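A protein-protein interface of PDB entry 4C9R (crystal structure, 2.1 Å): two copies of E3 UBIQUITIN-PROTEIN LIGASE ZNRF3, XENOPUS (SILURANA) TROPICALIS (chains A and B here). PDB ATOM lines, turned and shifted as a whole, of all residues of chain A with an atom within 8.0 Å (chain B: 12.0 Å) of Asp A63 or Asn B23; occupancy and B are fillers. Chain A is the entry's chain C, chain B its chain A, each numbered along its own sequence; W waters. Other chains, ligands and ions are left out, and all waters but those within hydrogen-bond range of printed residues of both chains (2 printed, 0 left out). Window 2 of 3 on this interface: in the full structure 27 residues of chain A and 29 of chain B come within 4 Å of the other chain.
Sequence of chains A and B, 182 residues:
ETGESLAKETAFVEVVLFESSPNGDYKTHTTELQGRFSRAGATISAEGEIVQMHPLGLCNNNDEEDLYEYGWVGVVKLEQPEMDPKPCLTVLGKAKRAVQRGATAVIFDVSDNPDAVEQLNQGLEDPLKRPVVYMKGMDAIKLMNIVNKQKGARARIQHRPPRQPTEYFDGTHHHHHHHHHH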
ATOM      1  N   CYS A  59      12.745  16.963 -19.745  1.00  0.00           N
ATOM      2  CA  CYS A  59      11.990  18.010 -19.062  1.00  0.00           C
ATOM      3  C   CYS A  59      10.498  17.667 -19.090  1.00  0.00           C
ATOM      4  O   CYS A  59      10.077  16.753 -19.794  1.00  0.00           O
ATOM      5  CB  CYS A  59      12.193  19.352 -19.764  1.00  0.00           C
ATOM      6  SG  CYS A  59      13.890  19.963 -19.721  1.00  0.00           S
ATOM      7  N   ASN A  60       9.714  18.393 -18.300  1.00  0.00           N
ATOM      8  CA  ASN A  60       8.264  18.460 -18.496  1.00  0.00           C
ATOM      9  C   ASN A  60       7.883  19.337 -19.695  1.00  0.00           C
ATOM     10  O   ASN A  60       6.955  19.005 -20.442  1.00  0.00           O
ATOM     11  CB  ASN A  60       7.590  18.946 -17.212  1.00  0.00           C
ATOM     12  CG  ASN A  60       7.632  17.900 -16.127  1.00  0.00           C
ATOM     13  OD1 ASN A  60       8.640  17.260 -15.918  1.00  0.00           O
ATOM     14  ND2 ASN A  60       6.517  17.683 -15.478  1.00  0.00           N
ATOM     15  N   ASN A  61       8.618  20.439 -19.871  1.00  0.00           N
ATOM     16  CA  ASN A  61       8.594  21.272 -21.094  1.00  0.00           C
ATOM     17  C   ASN A  61       8.956  20.509 -22.403  1.00  0.00           C
ATOM     18  O   ASN A  61       9.120  19.283 -22.392  1.00  0.00           O
ATOM     19  CB  ASN A  61       9.534  22.478 -20.907  1.00  0.00           C
ATOM     20  N   ASN A  62       9.085  21.249 -23.515  1.00  0.00           N
ATOM     21  CA  ASN A  62       9.192  20.679 -24.884  1.00  0.00           C
ATOM     22  C   ASN A  62       8.090  19.651 -25.160  1.00  0.00           C
ATOM     23  O   ASN A  62       8.281  18.705 -25.935  1.00  0.00           O
ATOM     24  CB  ASN A  62      10.573  20.056 -25.118  1.00  0.00           C
ATOM     25  N   ASP A  63       6.929  19.898 -24.545  1.00  0.00           N
ATOM     26  CA  ASP A  63       5.932  18.862 -24.217  1.00  0.00           C
ATOM     27  C   ASP A  63       5.747  17.783 -25.277  1.00  0.00           C
ATOM     28  O   ASP A  63       5.873  16.594 -24.977  1.00  0.00           O
ATOM     29  CB  ASP A  63       4.583  19.503 -23.851  1.00  0.00           C
ATOM     30  CG  ASP A  63       4.550  20.012 -22.414  1.00  0.00           C
ATOM     31  OD1 ASP A  63       5.574  20.543 -21.931  1.00  0.00           O
ATOM     32  OD2 ASP A  63       3.498  19.879 -21.761  1.00  0.00           O
ATOM     33  N   GLU A  64       5.457  18.192 -26.508  1.00  0.00           N
ATOM     34  CA  GLU A  64       5.362  17.243 -27.615  1.00  0.00           C
ATOM     35  C   GLU A  64       6.747  16.630 -27.914  1.00  0.00           C
ATOM     36  O   GLU A  64       7.405  17.010 -28.886  1.00  0.00           O
ATOM     37  CB  GLU A  64       4.776  17.931 -28.856  1.00  0.00           C
ATOM     38  N   GLU A  65       7.182  15.696 -27.063  1.00  0.00           N
ATOM     39  CA  GLU A  65       8.429  14.950 -27.278  1.00  0.00           C
ATOM     40  C   GLU A  65       8.098  13.684 -28.081  1.00  0.00           C
ATOM     41  O   GLU A  65       6.945  13.272 -28.142  1.00  0.00           O
ATOM     42  CB  GLU A  65       9.097  14.610 -25.936  1.00  0.00           C
ATOM     43  N   ASP A  66       9.094  13.064 -28.701  1.00  0.00           N
ATOM     44  CA  ASP A  66       8.852  11.890 -29.570  1.00  0.00           C
ATOM     45  C   ASP A  66       8.643  10.552 -28.831  1.00  0.00           C
ATOM     46  O   ASP A  66       8.863  10.442 -27.617  1.00  0.00           O
ATOM     47  CB  ASP A  66       9.988  11.749 -30.583  1.00  0.00           C
ATOM     48  CG  ASP A  66      10.024  12.892 -31.551  1.00  0.00           C
ATOM     49  OD1 ASP A  66       9.269  12.849 -32.549  1.00  0.00           O
ATOM     50  OD2 ASP A  66      10.788  13.848 -31.299  1.00  0.00           O
ATOM     51  N   LEU A  67       8.236   9.544 -29.593  1.00  0.00           N
ATOM     52  CA  LEU A  67       7.764   8.278 -29.038  1.00  0.00           C
ATOM     53  C   LEU A  67       8.713   7.132 -29.405  1.00  0.00           C
ATOM     54  O   LEU A  67       8.852   6.777 -30.575  1.00  0.00           O
ATOM     55  CB  LEU A  67       6.348   7.975 -29.559  1.00  0.00           C
ATOM     56  CG  LEU A  67       5.567   6.788 -28.951  1.00  0.00           C
ATOM     57  CD1 LEU A  67       5.185   7.066 -27.493  1.00  0.00           C
ATOM     58  CD2 LEU A  67       4.338   6.445 -29.800  1.00  0.00           C
ATOM     59  N   ARG A  97      11.459  10.915 -15.577  1.00  0.00           N
ATOM     60  CA  ARG A  97      10.899  11.283 -16.855  1.00  0.00           C
ATOM     61  C   ARG A  97      11.281  10.269 -17.955  1.00  0.00           C
ATOM     62  O   ARG A  97      10.487   9.943 -18.838  1.00  0.00           O
ATOM     63  CB  ARG A  97      11.412  12.650 -17.240  1.00  0.00           C
ATOM     64  CG  ARG A  97      10.791  13.219 -18.485  1.00  0.00           C
ATOM     65  CD  ARG A  97       9.479  13.939 -18.180  1.00  0.00           C
ATOM     66  NE  ARG A  97       8.805  14.194 -19.435  1.00  0.00           N
ATOM     67  CZ  ARG A  97       7.713  13.558 -19.875  1.00  0.00           C
ATOM     68  NH1 ARG A  97       7.064  12.673 -19.120  1.00  0.00           N
ATOM     69  NH2 ARG A  97       7.237  13.866 -21.063  1.00  0.00           N
ATOM     70  N   GLN A 100       8.951   7.408 -17.262  1.00  0.00           N
ATOM     71  CA  GLN A 100       7.652   7.759 -17.826  1.00  0.00           C
ATOM     72  C   GLN A 100       7.584   7.581 -19.313  1.00  0.00           C
ATOM     73  O   GLN A 100       6.542   7.189 -19.829  1.00  0.00           O
ATOM     74  CB  GLN A 100       7.264   9.201 -17.514  1.00  0.00           C
ATOM     75  CG  GLN A 100       6.860   9.446 -16.060  1.00  0.00           C
ATOM     76  CD  GLN A 100       6.983  10.936 -15.671  1.00  0.00           C
ATOM     77  OE1 GLN A 100       7.335  11.794 -16.482  1.00  0.00           O
ATOM     78  NE2 GLN A 100       6.698  11.227 -14.430  1.00  0.00           N
ATOM     79  N   ARG A 101       8.665   7.912 -20.011  1.00  0.00           N
ATOM     80  CA  ARG A 101       8.689   7.830 -21.445  1.00  0.00           C
ATOM     81  C   ARG A 101       9.155   6.466 -21.984  1.00  0.00           C
ATOM     82  O   ARG A 101       9.451   6.314 -23.188  1.00  0.00           O
ATOM     83  CB  ARG A 101       9.535   8.950 -22.019  1.00  0.00           C
ATOM     84  CG  ARG A 101       8.884  10.306 -21.791  1.00  0.00           C
ATOM     85  CD  ARG A 101       9.713  11.436 -22.355  1.00  0.00           C
ATOM     86  NE  ARG A 101      10.164  11.259 -23.751  1.00  0.00           N
ATOM     87  CZ  ARG A 101      11.205  11.907 -24.298  1.00  0.00           C
ATOM     88  NH1 ARG A 101      11.931  12.765 -23.591  1.00  0.00           N
ATOM     89  NH2 ARG A 101      11.535  11.691 -25.563  1.00  0.00           N
ATOM     90  N   GLU B  19       0.934   1.029 -22.824  1.00  0.00           N
ATOM     91  CA  GLU B  19       0.053   1.859 -23.603  1.00  0.00           C
ATOM     92  C   GLU B  19       0.536   3.302 -23.573  1.00  0.00           C
ATOM     93  O   GLU B  19       0.758   3.850 -22.502  1.00  0.00           O
ATOM     94  CB  GLU B  19      -1.356   1.790 -23.017  1.00  0.00           C
ATOM     95  CG  GLU B  19      -2.339   2.350 -23.990  1.00  0.00           C
ATOM     96  CD  GLU B  19      -1.994   1.909 -25.400  1.00  0.00           C
ATOM     97  OE1 GLU B  19      -2.319   0.746 -25.747  1.00  0.00           O
ATOM     98  OE2 GLU B  19      -1.373   2.711 -26.145  1.00  0.00           O
ATOM     99  N   SER B  20       0.690   3.918 -24.732  1.00  0.00           N
ATOM    100  CA  SER B  20       1.064   5.316 -24.750  1.00  0.00           C
ATOM    101  C   SER B  20      -0.139   6.105 -24.250  1.00  0.00           C
ATOM    102  O   SER B  20      -1.288   5.739 -24.493  1.00  0.00           O
ATOM    103  CB  SER B  20       1.465   5.764 -26.127  1.00  0.00           C
ATOM    104  OG  SER B  20       0.331   6.188 -26.812  1.00  0.00           O
ATOM    105  N   SER B  21       0.147   7.148 -23.488  1.00  0.00           N
ATOM    106  CA  SER B  21      -0.850   7.885 -22.728  1.00  0.00           C
ATOM    107  C   SER B  21      -0.679   9.334 -23.184  1.00  0.00           C
ATOM    108  O   SER B  21       0.199   9.592 -24.043  1.00  0.00           O
ATOM    109  CB  SER B  21      -0.651   7.663 -21.215  1.00  0.00           C
ATOM    110  OG  SER B  21       0.628   7.115 -20.942  1.00  0.00           O
ATOM    111  N   PRO B  22      -1.517  10.264 -22.654  1.00  0.00           N
ATOM    112  CA  PRO B  22      -1.755  11.572 -23.299  1.00  0.00           C
ATOM    113  C   PRO B  22      -0.549  12.299 -23.925  1.00  0.00           C
ATOM    114  O   PRO B  22      -0.643  12.782 -25.062  1.00  0.00           O
ATOM    115  CB  PRO B  22      -2.365  12.397 -22.157  1.00  0.00           C
ATOM    116  CG  PRO B  22      -3.163  11.389 -21.402  1.00  0.00           C
ATOM    117  CD  PRO B  22      -2.294  10.158 -21.397  1.00  0.00           C
ATOM    118  N   ASN B  23       0.579  12.319 -23.212  1.00  0.00           N
ATOM    119  CA  ASN B  23       1.698  13.229 -23.509  1.00  0.00           C
ATOM    120  C   ASN B  23       2.846  12.628 -24.316  1.00  0.00           C
ATOM    121  O   ASN B  23       3.598  13.354 -24.959  1.00  0.00           O
ATOM    122  CB  ASN B  23       2.237  13.840 -22.205  1.00  0.00           C
ATOM    123  CG  ASN B  23       1.708  13.143 -20.967  1.00  0.00           C
ATOM    124  OD1 ASN B  23       1.053  13.750 -20.128  1.00  0.00           O
ATOM    125  ND2 ASN B  23       1.972  11.863 -20.861  1.00  0.00           N
ATOM    126  N   GLY B  24       2.950  11.306 -24.329  1.00  0.00           N
ATOM    127  CA  GLY B  24       4.150  10.627 -24.818  1.00  0.00           C
ATOM    128  C   GLY B  24       4.673   9.678 -23.757  1.00  0.00           C
ATOM    129  O   GLY B  24       5.674   8.994 -23.962  1.00  0.00           O
ATOM    130  N   ASP B  25       3.995   9.658 -22.617  1.00  0.00           N
ATOM    131  CA  ASP B  25       4.298   8.742 -21.543  1.00  0.00           C
ATOM    132  C   ASP B  25       3.686   7.410 -21.881  1.00  0.00           C
ATOM    133  O   ASP B  25       2.971   7.282 -22.888  1.00  0.00           O
ATOM    134  CB  ASP B  25       3.694   9.227 -20.232  1.00  0.00           C
ATOM    135  CG  ASP B  25       4.351  10.470 -19.723  1.00  0.00           C
ATOM    136  OD1 ASP B  25       5.036  11.157 -20.524  1.00  0.00           O
ATOM    137  OD2 ASP B  25       4.191  10.762 -18.513  1.00  0.00           O
ATOM    138  N   TYR B  26       3.958   6.428 -21.034  1.00  0.00           N
ATOM    139  CA  TYR B  26       3.421   5.104 -21.193  1.00  0.00           C
ATOM    140  C   TYR B  26       2.761   4.785 -19.932  1.00  0.00           C
ATOM    141  O   TYR B  26       3.305   5.080 -18.893  1.00  0.00           O
ATOM    142  CB  TYR B  26       4.513   4.094 -21.387  1.00  0.00           C
ATOM    143  CG  TYR B  26       4.948   3.932 -22.800  1.00  0.00           C
ATOM    144  CD1 TYR B  26       4.204   3.195 -23.694  1.00  0.00           C
ATOM    145  CD2 TYR B  26       6.126   4.487 -23.229  1.00  0.00           C
ATOM    146  CE1 TYR B  26       4.618   3.042 -25.005  1.00  0.00           C
ATOM    147  CE2 TYR B  26       6.554   4.345 -24.533  1.00  0.00           C
ATOM    148  CZ  TYR B  26       5.816   3.604 -25.406  1.00  0.00           C
ATOM    149  OH  TYR B  26       6.283   3.469 -26.686  1.00  0.00           O
ATOM    150  N   LYS B  27       1.574   4.202 -20.033  1.00  0.00           N
ATOM    151  CA  LYS B  27       0.874   3.573 -18.918  1.00  0.00           C
ATOM    152  C   LYS B  27       1.126   2.058 -19.063  1.00  0.00           C
ATOM    153  O   LYS B  27       1.048   1.508 -20.164  1.00  0.00           O
ATOM    154  CB  LYS B  27      -0.614   3.890 -19.043  1.00  0.00           C
ATOM    155  CG  LYS B  27      -1.515   3.218 -18.019  1.00  0.00           C
ATOM    156  CD  LYS B  27      -2.911   3.845 -18.049  1.00  0.00           C
ATOM    157  CE  LYS B  27      -3.838   3.278 -16.980  1.00  0.00           C
ATOM    158  NZ  LYS B  27      -5.228   3.785 -17.181  1.00  0.00           N
ATOM    159  N   THR B  28       1.485   1.404 -17.976  1.00  0.00           N
ATOM    160  CA  THR B  28       1.869   0.028 -18.046  1.00  0.00           C
ATOM    161  C   THR B  28       1.070  -0.743 -17.053  1.00  0.00           C
ATOM    162  O   THR B  28       0.718  -0.225 -16.018  1.00  0.00           O
ATOM    163  CB  THR B  28       3.356  -0.187 -17.749  1.00  0.00           C
ATOM    164  OG1 THR B  28       3.662   0.270 -16.432  1.00  0.00           O
ATOM    165  CG2 THR B  28       4.223   0.575 -18.748  1.00  0.00           C
HETATM  166  O   HOH W   1       7.876   7.808 -25.408  1.00  0.00           O
HETATM  167  O   HOH W   2       7.757  10.789 -24.859  1.00  0.00           O
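Among the printed residues, merely in contact across the chains: Gln A100 with Asp B25 (3.2 Å), Arg A101 with Tyr B26 (3.8 Å), Leu A67 with Tyr B26 (3.8 Å) and Asp A63 with Asn B23 (3.96 Å).
Printed residues of chain A that touch a printed residue of chain B: Asp A63, Leu A67, Arg A97, Gln A100 and Arg A101.
Hydrophobic or aromatic side chains of chain A that line the printed part of chain B: Leu A67.
Hydrophobic or aromatic side chains of chain B within 4 Å of the printed part of chain A: Tyr B26.
Along chain B the printed residues that touch a printed residue of chain A span positions 23 to 26.
Among the printed residues, Asp or Glu carboxylates within 4 Å of a Lys or Arg side-chain nitrogen of the other chain: Arg A97 with Asp B25.
No position is printed for both chains.
Of the 6 pairs that touch across the chains among the printed residues, none has its exchanged pair printed and touching as well.
The side-chain carboxylate (OD1) of Asp B25 is in salt-bridge range of the guanidinium group (NH1) of Arg A97 (2.9 Å).
The backbone NH (N) of Tyr B26 sits at hydrogen-bond distance from the backbone carbonyl oxygen (O) of Gln A100 (3.0 Å).
Water W2 lies within hydrogen-bond range of the guanidinium group (NE) of Arg A101 (2.7 Å), the backbone carbonyl oxygen (O) of Gly B24 (2.9 Å) and the backbone carbonyl oxygen (O) of Asp A66 (3.0 Å).
Water W1 lies within hydrogen-bond range of the backbone carbonyl oxygen (O) of Gly B24 (2.9 Å) and the backbone carbonyl oxygen (O) of Arg A101 (3.1 Å).
The side-chain hydroxyl (OG) of Ser B21 sits at hydrogen-bond distance from the backbone carbonyl oxygen (O) of Asp B25 (3.1 Å).
The side-chain hydroxyl of Ser B21 sits close to the backbone NH of Tyr B26 (3.4 Å).
ND2 of Asn B23 sits close to OD1 of Asp B25, at 3.2 Å.
O of Cys A59 is in hydrogen-bond range of NE of Arg A97 (2.9 Å).
The side-chain carboxylate of Asp A63 lies close to the backbone carbonyl oxygen of Asn A60 (2.5 Å).
The guanidinium group (NH1) of Arg A97 lies within hydrogen-bond range of the side-chain amide oxygen (OE1) of Gln A100.
No residue of chain B comes within 4 Å of Asn A60.
No residue of chain B comes within 4 Å of Asn A62.
Asp A63 touches one residue of chain B.
Glu A64 touches none of the printed residues of chain B.
Glu A65 touches none of the printed residues of chain B.
Of the printed residues of chain B, Leu A67 touches Tyr B26 (3.8 Å).
Of the printed residues of chain B, Arg A97 touches Asp B25 (2.9 Å).
Of the printed residues of chain A, Asp B25 touches Arg A97 and Gln A100.
The nearest residue of chain B that does not touch Asp A63 is Gly B24 (6.1 Å).
The nearest residue of chain A that does not touch Asn B23 is Glu A65 (4.6 Å).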
